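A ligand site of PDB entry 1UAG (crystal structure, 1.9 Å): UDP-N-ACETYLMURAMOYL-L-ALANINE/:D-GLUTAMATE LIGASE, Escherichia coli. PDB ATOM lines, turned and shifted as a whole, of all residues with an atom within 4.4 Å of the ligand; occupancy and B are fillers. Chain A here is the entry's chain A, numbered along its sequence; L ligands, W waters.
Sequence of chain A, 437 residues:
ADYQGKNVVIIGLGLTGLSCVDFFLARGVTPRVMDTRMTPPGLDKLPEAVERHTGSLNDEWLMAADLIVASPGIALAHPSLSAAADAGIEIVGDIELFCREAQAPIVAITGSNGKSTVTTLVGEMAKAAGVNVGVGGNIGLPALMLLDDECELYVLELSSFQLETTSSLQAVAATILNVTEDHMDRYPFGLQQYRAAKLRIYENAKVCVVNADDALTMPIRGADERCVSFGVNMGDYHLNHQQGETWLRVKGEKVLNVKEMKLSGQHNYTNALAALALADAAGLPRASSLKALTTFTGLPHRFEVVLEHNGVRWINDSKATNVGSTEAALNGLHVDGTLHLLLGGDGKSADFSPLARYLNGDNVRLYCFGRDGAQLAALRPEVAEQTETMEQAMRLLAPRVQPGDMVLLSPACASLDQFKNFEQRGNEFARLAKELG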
ATOM      1  N   ILE A  11      -0.294 -20.961  16.533  1.00  0.00           N
ATOM      2  CA  ILE A  11      -0.345 -20.707  17.971  1.00  0.00           C
ATOM      3  C   ILE A  11       1.083 -20.531  18.491  1.00  0.00           C
ATOM      4  O   ILE A  11       1.932 -21.401  18.321  1.00  0.00           O
ATOM      5  CB  ILE A  11      -1.022 -21.842  18.741  1.00  0.00           C
ATOM      6  CG1 ILE A  11      -2.382 -22.134  18.151  1.00  0.00           C
ATOM      7  CG2 ILE A  11      -1.127 -21.458  20.228  1.00  0.00           C
ATOM      8  CD1 ILE A  11      -3.051 -23.360  18.750  1.00  0.00           C
ATOM      9  N   GLY A  12       1.329 -19.373  19.109  1.00  0.00           N
ATOM     10  CA  GLY A  12       2.617 -19.096  19.686  1.00  0.00           C
ATOM     11  C   GLY A  12       3.272 -17.913  19.032  1.00  0.00           C
ATOM     12  O   GLY A  12       3.462 -17.881  17.820  1.00  0.00           O
ATOM     13  N   GLY A  14       6.291 -16.751  20.028  1.00  0.00           N
ATOM     14  CA  GLY A  14       7.652 -16.715  20.490  1.00  0.00           C
ATOM     15  C   GLY A  14       8.584 -16.818  19.297  1.00  0.00           C
ATOM     16  O   GLY A  14       8.206 -16.445  18.191  1.00  0.00           O
ATOM     17  N   LEU A  15       9.721 -17.489  19.500  1.00  0.00           N
ATOM     18  CA  LEU A  15      10.666 -17.750  18.432  1.00  0.00           C
ATOM     19  C   LEU A  15      10.071 -18.624  17.324  1.00  0.00           C
ATOM     20  O   LEU A  15      10.278 -18.358  16.149  1.00  0.00           O
ATOM     21  CB  LEU A  15      11.913 -18.424  18.986  1.00  0.00           C
ATOM     22  CG  LEU A  15      12.706 -17.657  20.038  1.00  0.00           C
ATOM     23  CD1 LEU A  15      13.886 -18.515  20.475  1.00  0.00           C
ATOM     24  CD2 LEU A  15      13.184 -16.337  19.444  1.00  0.00           C
ATOM     25  N   THR A  16       9.429 -19.726  17.711  1.00  0.00           N
ATOM     26  CA  THR A  16       8.849 -20.648  16.757  1.00  0.00           C
ATOM     27  C   THR A  16       7.769 -19.992  15.935  1.00  0.00           C
ATOM     28  O   THR A  16       7.793 -20.058  14.714  1.00  0.00           O
ATOM     29  CB  THR A  16       8.232 -21.879  17.447  1.00  0.00           C
ATOM     30  OG1 THR A  16       9.216 -22.503  18.275  1.00  0.00           O
ATOM     31  CG2 THR A  16       7.732 -22.902  16.401  1.00  0.00           C
ATOM     32  N   ASP A  35      -1.855 -16.361  20.804  1.00  0.00           N
ATOM     33  CA  ASP A  35      -1.018 -16.766  21.936  1.00  0.00           C
ATOM     34  C   ASP A  35      -1.835 -16.487  23.180  1.00  0.00           C
ATOM     35  O   ASP A  35      -2.617 -15.523  23.208  1.00  0.00           O
ATOM     36  CB  ASP A  35       0.274 -15.941  21.937  1.00  0.00           C
ATOM     37  CG  ASP A  35       1.350 -16.541  22.824  1.00  0.00           C
ATOM     38  OD1 ASP A  35       1.137 -16.682  24.042  1.00  0.00           O
ATOM     39  OD2 ASP A  35       2.418 -16.859  22.287  1.00  0.00           O
ATOM     40  N   THR A  36      -1.765 -17.383  24.163  1.00  0.00           N
ATOM     41  CA  THR A  36      -2.542 -17.186  25.383  1.00  0.00           C
ATOM     42  C   THR A  36      -1.913 -16.133  26.304  1.00  0.00           C
ATOM     43  O   THR A  36      -2.600 -15.578  27.150  1.00  0.00           O
ATOM     44  CB  THR A  36      -2.756 -18.507  26.179  1.00  0.00           C
ATOM     45  OG1 THR A  36      -1.523 -18.975  26.726  1.00  0.00           O
ATOM     46  CG2 THR A  36      -3.377 -19.597  25.286  1.00  0.00           C
ATOM     47  N   ARG A  37      -0.637 -15.818  26.098  1.00  0.00           N
ATOM     48  CA  ARG A  37       0.026 -14.737  26.839  1.00  0.00           C
ATOM     49  C   ARG A  37      -0.516 -13.426  26.332  1.00  0.00           C
ATOM     50  O   ARG A  37      -0.720 -13.256  25.137  1.00  0.00           O
ATOM     51  CB  ARG A  37       1.532 -14.768  26.630  1.00  0.00           C
ATOM     52  CG  ARG A  37       2.223 -15.976  27.253  1.00  0.00           C
ATOM     53  CD  ARG A  37       3.649 -16.108  26.787  1.00  0.00           C
ATOM     54  NE  ARG A  37       3.748 -16.490  25.392  1.00  0.00           N
ATOM     55  CZ  ARG A  37       4.889 -16.800  24.788  1.00  0.00           C
ATOM     56  NH1 ARG A  37       6.025 -16.744  25.459  1.00  0.00           N
ATOM     57  NH2 ARG A  37       4.902 -17.272  23.547  1.00  0.00           N
ATOM     58  N   SER A  71       3.074 -24.087  18.192  1.00  0.00           N
ATOM     59  CA  SER A  71       4.412 -23.987  18.790  1.00  0.00           C
ATOM     60  C   SER A  71       4.532 -25.030  19.915  1.00  0.00           C
ATOM     61  O   SER A  71       3.538 -25.408  20.556  1.00  0.00           O
ATOM     62  CB  SER A  71       4.647 -22.577  19.376  1.00  0.00           C
ATOM     63  OG  SER A  71       4.835 -21.597  18.341  1.00  0.00           O
ATOM     64  N   PRO A  72       5.762 -25.454  20.244  1.00  0.00           N
ATOM     65  CA  PRO A  72       5.917 -26.523  21.230  1.00  0.00           C
ATOM     66  C   PRO A  72       5.424 -26.134  22.608  1.00  0.00           C
ATOM     67  O   PRO A  72       5.114 -27.001  23.408  1.00  0.00           O
ATOM     68  CB  PRO A  72       7.415 -26.808  21.209  1.00  0.00           C
ATOM     69  CG  PRO A  72       8.017 -25.513  20.742  1.00  0.00           C
ATOM     70  CD  PRO A  72       7.059 -25.010  19.714  1.00  0.00           C
ATOM     71  N   GLY A  73       5.296 -24.828  22.847  1.00  0.00           N
ATOM     72  CA  GLY A  73       4.917 -24.321  24.161  1.00  0.00           C
ATOM     73  C   GLY A  73       3.422 -24.345  24.453  1.00  0.00           C
ATOM     74  O   GLY A  73       3.013 -23.923  25.524  1.00  0.00           O
ATOM     75  N   ILE A  74       2.596 -24.797  23.505  1.00  0.00           N
ATOM     76  CA  ILE A  74       1.156 -24.988  23.770  1.00  0.00           C
ATOM     77  C   ILE A  74       0.857 -26.481  23.779  1.00  0.00           C
ATOM     78  O   ILE A  74       1.307 -27.216  22.894  1.00  0.00           O
ATOM     79  CB  ILE A  74       0.252 -24.222  22.697  1.00  0.00           C
ATOM     80  CG1 ILE A  74      -1.224 -24.215  23.134  1.00  0.00           C
ATOM     81  CG2 ILE A  74       0.359 -24.900  21.321  1.00  0.00           C
ATOM     82  CD1 ILE A  74      -1.616 -23.137  24.144  1.00  0.00           C
ATOM     83  N   LYS A 115      21.339 -33.287  25.245  1.00  0.00           N
ATOM     84  CA  LYS A 115      20.774 -32.964  23.925  1.00  0.00           C
ATOM     85  C   LYS A 115      21.593 -31.946  23.116  1.00  0.00           C
ATOM     86  O   LYS A 115      21.921 -32.185  21.957  1.00  0.00           O
ATOM     87  CB  LYS A 115      19.349 -32.406  24.089  1.00  0.00           C
ATOM     88  CG  LYS A 115      18.250 -33.396  24.260  1.00  0.00           C
ATOM     89  CD  LYS A 115      16.856 -32.784  23.865  1.00  0.00           C
ATOM     90  CE  LYS A 115      16.469 -31.535  24.637  1.00  0.00           C
ATOM     91  NZ  LYS A 115      16.519 -31.694  26.121  1.00  0.00           N
ATOM     92  N   GLY A 137      16.773 -26.294  15.899  1.00  0.00           N
ATOM     93  CA  GLY A 137      15.720 -26.987  16.620  1.00  0.00           C
ATOM     94  C   GLY A 137      15.628 -26.420  18.013  1.00  0.00           C
ATOM     95  O   GLY A 137      15.913 -25.231  18.204  1.00  0.00           O
ATOM     96  N   ASN A 138      15.422 -27.297  18.995  1.00  0.00           N
ATOM     97  CA  ASN A 138      15.192 -26.884  20.377  1.00  0.00           C
ATOM     98  C   ASN A 138      16.440 -26.229  20.963  1.00  0.00           C
ATOM     99  O   ASN A 138      16.354 -25.481  21.938  1.00  0.00           O
ATOM    100  CB  ASN A 138      14.790 -28.104  21.213  1.00  0.00           C
ATOM    101  CG  ASN A 138      14.343 -27.735  22.612  1.00  0.00           C
ATOM    102  OD1 ASN A 138      13.297 -27.099  22.795  1.00  0.00           O
ATOM    103  ND2 ASN A 138      15.081 -28.190  23.618  1.00  0.00           N
ATOM    104  N   ILE A 139      17.590 -26.498  20.364  1.00  0.00           N
ATOM    105  CA  ILE A 139      18.848 -25.875  20.774  1.00  0.00           C
ATOM    106  C   ILE A 139      18.785 -24.336  20.708  1.00  0.00           C
ATOM    107  O   ILE A 139      19.492 -23.636  21.431  1.00  0.00           O
ATOM    108  CB  ILE A 139      20.042 -26.415  19.910  1.00  0.00           C
ATOM    109  CG1 ILE A 139      21.392 -26.047  20.555  1.00  0.00           C
ATOM    110  CG2 ILE A 139      19.975 -25.886  18.498  1.00  0.00           C
ATOM    111  CD1 ILE A 139      22.541 -26.898  20.065  1.00  0.00           C
ATOM    112  N   GLY A 140      17.893 -23.817  19.868  1.00  0.00           N
ATOM    113  CA  GLY A 140      17.552 -22.401  19.950  1.00  0.00           C
ATOM    114  C   GLY A 140      17.299 -21.708  18.633  1.00  0.00           C
ATOM    115  O   GLY A 140      16.729 -20.633  18.609  1.00  0.00           O
ATOM    116  N   PRO A 142      15.352 -21.755  15.301  1.00  0.00           N
ATOM    117  CA  PRO A 142      14.168 -22.419  14.743  1.00  0.00           C
ATOM    118  C   PRO A 142      14.517 -23.155  13.453  1.00  0.00           C
ATOM    119  O   PRO A 142      15.205 -22.630  12.592  1.00  0.00           O
ATOM    120  CB  PRO A 142      13.192 -21.266  14.518  1.00  0.00           C
ATOM    121  CG  PRO A 142      13.531 -20.323  15.588  1.00  0.00           C
ATOM    122  CD  PRO A 142      15.048 -20.340  15.620  1.00  0.00           C
ATOM    123  N   SER A 159      12.672 -31.572  21.271  1.00  0.00           N
ATOM    124  CA  SER A 159      12.079 -31.819  22.573  1.00  0.00           C
ATOM    125  C   SER A 159      10.919 -32.808  22.410  1.00  0.00           C
ATOM    126  O   SER A 159      10.422 -33.022  21.298  1.00  0.00           O
ATOM    127  CB  SER A 159      11.537 -30.522  23.169  1.00  0.00           C
ATOM    128  OG  SER A 159      10.574 -29.949  22.308  1.00  0.00           O
ATOM    129  N   PHE A 161       8.019 -32.066  23.199  1.00  0.00           N
ATOM    130  CA  PHE A 161       6.907 -31.204  22.764  1.00  0.00           C
ATOM    131  C   PHE A 161       6.866 -31.125  21.248  1.00  0.00           C
ATOM    132  O   PHE A 161       5.790 -31.266  20.637  1.00  0.00           O
ATOM    133  CB  PHE A 161       7.051 -29.784  23.307  1.00  0.00           C
ATOM    134  CG  PHE A 161       7.046 -29.675  24.813  1.00  0.00           C
ATOM    135  CD1 PHE A 161       6.458 -30.634  25.620  1.00  0.00           C
ATOM    136  CD2 PHE A 161       7.602 -28.542  25.417  1.00  0.00           C
ATOM    137  CE1 PHE A 161       6.403 -30.489  26.990  1.00  0.00           C
ATOM    138  CE2 PHE A 161       7.555 -28.382  26.812  1.00  0.00           C
ATOM    139  CZ  PHE A 161       6.959 -29.356  27.595  1.00  0.00           C
ATOM    140  N   GLN A 162       8.034 -30.869  20.650  1.00  0.00           N
ATOM    141  CA  GLN A 162       8.179 -30.826  19.194  1.00  0.00           C
ATOM    142  C   GLN A 162       7.852 -32.147  18.504  1.00  0.00           C
ATOM    143  O   GLN A 162       7.220 -32.157  17.457  1.00  0.00           O
ATOM    144  CB  GLN A 162       9.595 -30.441  18.822  1.00  0.00           C
ATOM    145  CG  GLN A 162       9.892 -28.979  19.037  1.00  0.00           C
ATOM    146  CD  GLN A 162      11.373 -28.699  18.997  1.00  0.00           C
ATOM    147  OE1 GLN A 162      12.172 -29.527  19.394  1.00  0.00           O
ATOM    148  NE2 GLN A 162      11.754 -27.529  18.520  1.00  0.00           N
ATOM    149  N   ASP A 182      10.780 -34.890  33.573  1.00  0.00           N
ATOM    150  CA  ASP A 182      10.787 -33.483  33.192  1.00  0.00           C
ATOM    151  C   ASP A 182       9.456 -33.169  32.562  1.00  0.00           C
ATOM    152  O   ASP A 182       8.743 -34.083  32.161  1.00  0.00           O
ATOM    153  CB  ASP A 182      11.922 -33.208  32.211  1.00  0.00           C
ATOM    154  CG  ASP A 182      12.261 -31.730  32.111  1.00  0.00           C
ATOM    155  OD1 ASP A 182      11.685 -30.885  32.830  1.00  0.00           O
ATOM    156  OD2 ASP A 182      13.151 -31.402  31.293  1.00  0.00           O
ATOM    157  N   HIS A 183       9.057 -31.899  32.652  1.00  0.00           N
ATOM    158  CA  HIS A 183       7.850 -31.382  31.976  1.00  0.00           C
ATOM    159  C   HIS A 183       6.575 -32.076  32.460  1.00  0.00           C
ATOM    160  O   HIS A 183       5.640 -32.304  31.670  1.00  0.00           O
ATOM    161  CB  HIS A 183       7.967 -31.557  30.460  1.00  0.00           C
ATOM    162  CG  HIS A 183       9.136 -30.838  29.858  1.00  0.00           C
ATOM    163  ND1 HIS A 183       9.329 -29.502  30.060  1.00  0.00           N
ATOM    164  CD2 HIS A 183      10.133 -31.334  29.093  1.00  0.00           C
ATOM    165  CE1 HIS A 183      10.445 -29.196  29.429  1.00  0.00           C
ATOM    166  NE2 HIS A 183      10.967 -30.268  28.816  1.00  0.00           N
ATOM    167  N   LEU A 416      11.584 -19.711  33.927  1.00  0.00           N
ATOM    168  CA  LEU A 416      10.520 -18.891  33.330  1.00  0.00           C
ATOM    169  C   LEU A 416       9.727 -18.069  34.347  1.00  0.00           C
ATOM    170  O   LEU A 416       9.070 -17.095  33.978  1.00  0.00           O
ATOM    171  CB  LEU A 416       9.549 -19.772  32.553  1.00  0.00           C
ATOM    172  CG  LEU A 416       8.532 -20.536  33.435  1.00  0.00           C
ATOM    173  CD1 LEU A 416       7.217 -20.733  32.700  1.00  0.00           C
ATOM    174  CD2 LEU A 416       9.124 -21.853  33.853  1.00  0.00           C
ATOM    175  N   PHE A 422      16.975 -19.446  30.348  1.00  0.00           N
ATOM    176  CA  PHE A 422      18.054 -19.930  31.203  1.00  0.00           C
ATOM    177  C   PHE A 422      19.329 -19.210  30.879  1.00  0.00           C
ATOM    178  O   PHE A 422      20.178 -19.038  31.742  1.00  0.00           O
ATOM    179  CB  PHE A 422      18.233 -21.456  31.107  1.00  0.00           C
ATOM    180  CG  PHE A 422      18.830 -21.929  29.813  1.00  0.00           C
ATOM    181  CD1 PHE A 422      20.210 -21.838  29.578  1.00  0.00           C
ATOM    182  CD2 PHE A 422      18.012 -22.424  28.811  1.00  0.00           C
ATOM    183  CE1 PHE A 422      20.755 -22.229  28.350  1.00  0.00           C
ATOM    184  CE2 PHE A 422      18.548 -22.825  27.581  1.00  0.00           C
ATOM    185  CZ  PHE A 422      19.916 -22.713  27.344  1.00  0.00           C
HETATM  186  N1  LIG L   1       3.141 -20.058  25.836  1.00  0.00           N
HETATM  187  C1  LIG L   1       1.888 -19.742  26.373  1.00  0.00           C
HETATM  188  N2  LIG L   1       0.827 -19.833  25.494  1.00  0.00           N
HETATM  189  C2  LIG L   1       0.947 -19.968  24.110  1.00  0.00           C
HETATM  190  C3  LIG L   1       2.268 -20.328  23.638  1.00  0.00           C
HETATM  191  C4  LIG L   1       3.297 -20.361  24.499  1.00  0.00           C
HETATM  192  O1  LIG L   1       1.713 -19.470  27.566  1.00  0.00           O
HETATM  193  O2  LIG L   1       0.013 -19.679  23.373  1.00  0.00           O
HETATM  194  C5  LIG L   1       4.295 -20.127  26.781  1.00  0.00           C
HETATM  195  C6  LIG L   1       4.777 -21.552  26.856  1.00  0.00           C
HETATM  196  O3  LIG L   1       4.038 -22.409  27.820  1.00  0.00           O
HETATM  197  C7  LIG L   1       6.203 -21.528  27.205  1.00  0.00           C
HETATM  198  C8  LIG L   1       6.593 -20.264  26.467  1.00  0.00           C
HETATM  199  O4  LIG L   1       5.413 -19.552  26.156  1.00  0.00           O
HETATM  200  O5  LIG L   1       6.129 -21.385  28.648  1.00  0.00           O
HETATM  201  C9  LIG L   1       7.349 -20.464  25.224  1.00  0.00           C
HETATM  202  O6  LIG L   1       6.634 -21.206  24.318  1.00  0.00           O
HETATM  203  P1  LIG L   1       6.842 -21.052  22.747  1.00  0.00           P
HETATM  204  O7  LIG L   1       6.255 -22.270  22.161  1.00  0.00           O
HETATM  205  O8  LIG L   1       6.372 -19.796  22.298  1.00  0.00           O
HETATM  206  O9  LIG L   1       8.446 -21.144  22.672  1.00  0.00           O
HETATM  207  P2  LIG L   1       9.509 -20.488  21.657  1.00  0.00           P
HETATM  208  O10 LIG L   1       9.986 -19.175  22.067  1.00  0.00           O
HETATM  209  O11 LIG L   1       9.120 -20.713  20.277  1.00  0.00           O
HETATM  210  O12 LIG L   1      10.660 -21.636  21.899  1.00  0.00           O
HETATM  211  C10 LIG L   1      10.577 -22.996  21.506  1.00  0.00           C
HETATM  212  C11 LIG L   1      11.195 -23.860  22.560  1.00  0.00           C
HETATM  213  N3  LIG L   1      10.507 -23.719  23.848  1.00  0.00           N
HETATM  214  C12 LIG L   1       9.598 -24.616  24.247  1.00  0.00           C
HETATM  215  O13 LIG L   1       9.497 -25.702  23.692  1.00  0.00           O
HETATM  216  C13 LIG L   1       8.782 -24.327  25.489  1.00  0.00           C
HETATM  217  C14 LIG L   1      12.636 -23.446  22.684  1.00  0.00           C
HETATM  218  O14 LIG L   1      13.293 -24.308  23.629  1.00  0.00           O
HETATM  219  C15 LIG L   1      13.336 -23.602  21.335  1.00  0.00           C
HETATM  220  O15 LIG L   1      14.699 -23.267  21.437  1.00  0.00           O
HETATM  221  C16 LIG L   1      12.658 -22.751  20.286  1.00  0.00           C
HETATM  222  O16 LIG L   1      11.248 -23.108  20.247  1.00  0.00           O
HETATM  223  C17 LIG L   1      13.180 -23.069  18.916  1.00  0.00           C
HETATM  224  O17 LIG L   1      12.845 -24.417  18.599  1.00  0.00           O
HETATM  225  C18 LIG L   1      13.665 -23.987  24.971  1.00  0.00           C
HETATM  226  C19 LIG L   1      13.065 -24.866  26.035  1.00  0.00           C
HETATM  227  O18 LIG L   1      12.903 -24.457  27.158  1.00  0.00           O
HETATM  228  C20 LIG L   1      15.085 -23.408  25.083  1.00  0.00           C
HETATM  229  N4  LIG L   1      12.619 -26.043  25.603  1.00  0.00           N
HETATM  230  C21 LIG L   1      12.223 -27.119  26.484  1.00  0.00           C
HETATM  231  C22 LIG L   1      13.386 -28.025  26.974  1.00  0.00           C
HETATM  232  O19 LIG L   1      14.453 -28.013  26.303  1.00  0.00           O
HETATM  233  O20 LIG L   1      13.190 -28.781  27.951  1.00  0.00           O
HETATM  234  C23 LIG L   1      11.137 -27.982  25.826  1.00  0.00           C
HETATM  235  O   HOH W   1      12.699 -25.358  15.874  1.00  0.00           O
HETATM  236  O   HOH W   2      10.067 -25.185  17.808  1.00  0.00           O
HETATM  237  O   HOH W   3       8.587 -17.210  23.879  1.00  0.00           O
HETATM  238  O   HOH W   4      13.907 -28.966  30.704  1.00  0.00           O
HETATM  239  O   HOH W   5      10.903 -21.221  25.383  1.00  0.00           O
HETATM  240  O   HOH W   6      -0.589 -17.979  29.465  1.00  0.00           O
HETATM  241  O   HOH W   7      10.755 -27.324  22.009  1.00  0.00           O
HETATM  242  O   HOH W   8      13.925 -32.024  28.535  1.00  0.00           O
HETATM  243  O   HOH W   9      17.809 -25.350  24.337  1.00  0.00           O
HETATM  244  O   HOH W  10      16.152 -26.079  28.310  1.00  0.00           O
HETATM  245  O   HOH W  11       6.118 -19.524  19.420  1.00  0.00           O
HETATM  246  O   HOH W  12       4.260 -25.533  28.106  1.00  0.00           O
HETATM  247  O   HOH W  13      16.444 -20.687  26.100  1.00  0.00           O
HETATM  248  O   HOH W  14      12.656 -31.068  26.644  1.00  0.00           O
HETATM  249  O   HOH W  15      12.173 -19.102  24.099  1.00  0.00           O
HETATM  250  O   HOH W  16      15.319 -20.692  22.602  1.00  0.00           O
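An oxygen (O11) of the ligand sits at hydrogen-bond distance from the backbone NH of Thr 16, at 2.8 Å.
The side-chain hydroxyl (OG1) of Thr 16 lies within hydrogen-bond range of an oxygen (O11) of the ligand.
An oxygen (O15) of the ligand is in hydrogen-bond range of the backbone carbonyl oxygen (O) of Asn 138 (2.8 Å).
ND2 of Asn 138 is in hydrogen-bond range of O19 of the ligand (2.8 Å).
N of Thr 36 sits at hydrogen-bond distance from O2 of the ligand (3.0 Å).
OG1 of Thr 36 is in hydrogen-bond range of N2 of the ligand.
A ring nitrogen (NE2) of His 183 sits at hydrogen-bond distance from an oxygen (O20) of the ligand, 2.8 Å away.
An oxygen (O7) of the ligand lies within hydrogen-bond range of the backbone NH (N) of Gly 73, at 2.8 Å.
The backbone carbonyl oxygen (O) of Gly 73 sits at hydrogen-bond distance from an oxygen (O3) of the ligand, at 2.9 Å.
NH2 of Arg 37 lies within salt-bridge range of O8 of the ligand, 3.2 Å away.
The backbone NH (N) of Leu 15 is in hydrogen-bond range of an oxygen (O10) of the ligand, 3.1 Å away.
An oxygen (O17) of the ligand sits at hydrogen-bond distance from the backbone carbonyl oxygen of Gly 137, at 3.2 Å.
N2 of the ligand lies close to OD1 of Asp 35 (3.5 Å).
NE2 of Gln 162 is in hydrogen-bond range of O17 of the ligand (3.3 Å).
A ring nitrogen (NE2) of His 183 lies within hydrogen-bond range of the side-chain carboxylate of Asp 182 (3.5 Å).
The guanidinium group (NH2) of Arg 37 lies within salt-bridge range of the side-chain carboxylate (OD2) of Asp 35, 2.8 Å away.
The backbone carbonyl oxygen of Ile 11 sits at hydrogen-bond distance from the side-chain hydroxyl of Ser 71, at 2.9 Å.
The side-chain amide oxygen (OE1) of Gln 162 lies within hydrogen-bond range of the backbone NH (N) of Ser 159.
The backbone NH (N) of Phe 161 lies close to the side-chain hydroxyl (OG) of Ser 159.
CG2 of Ile 11 touches O2 of the ligand, 3.8 Å away.
CA of Gly 14 touches O10 of the ligand, at 3.7 Å.
Ser 71 touches the ligand.
CG of Pro 72 touches O13 of the ligand, 3.3 Å away.
Ile 74 touches the ligand.
Gly 140 touches the ligand.
Ser 159 touches the ligand.
Phe 161 touches the ligand.
Hydrophobic or aromatic side chains that line the ligand: Ile 11, Leu 15, Pro 72, Ile 74, Phe 161 and His 183.
Of the 25 residues printed, 18 come within 4 Å of the ligand.
The nearest printed residue that does not touch the ligand is Gly 12 (4.2 Å).
Water W7 lies within hydrogen-bond range of the side-chain hydroxyl of Ser 159 (2.6 Å), an oxygen (O13) of the ligand (2.7 Å) and the side-chain amide oxygen of Asn 138 (2.7 Å).
Water W4 lies within hydrogen-bond range of OD2 of Asp 182 (2.6 Å) and O20 of the ligand (2.9 Å).
Water W11 lies within hydrogen-bond range of the side-chain hydroxyl (OG) of Ser 71 (2.7 Å), the backbone NH (N) of Gly 14 (2.8 Å) and an oxygen (O8) of the ligand (2.9 Å).
Water W12 bridges O3 of the ligand (3.1 Å) and O of Gly 73 (3.3 Å).
Water W6 bridges OG1 of Thr 36 (3.1 Å) and O1 of the ligand (3.3 Å).
Water W8 lies within hydrogen-bond range of the side-chain carboxylate (OD2) of Asp 182 (2.9 Å), an oxygen (O20) of the ligand (3.4 Å) and a ring nitrogen (NE2) of His 183 (3.5 Å).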
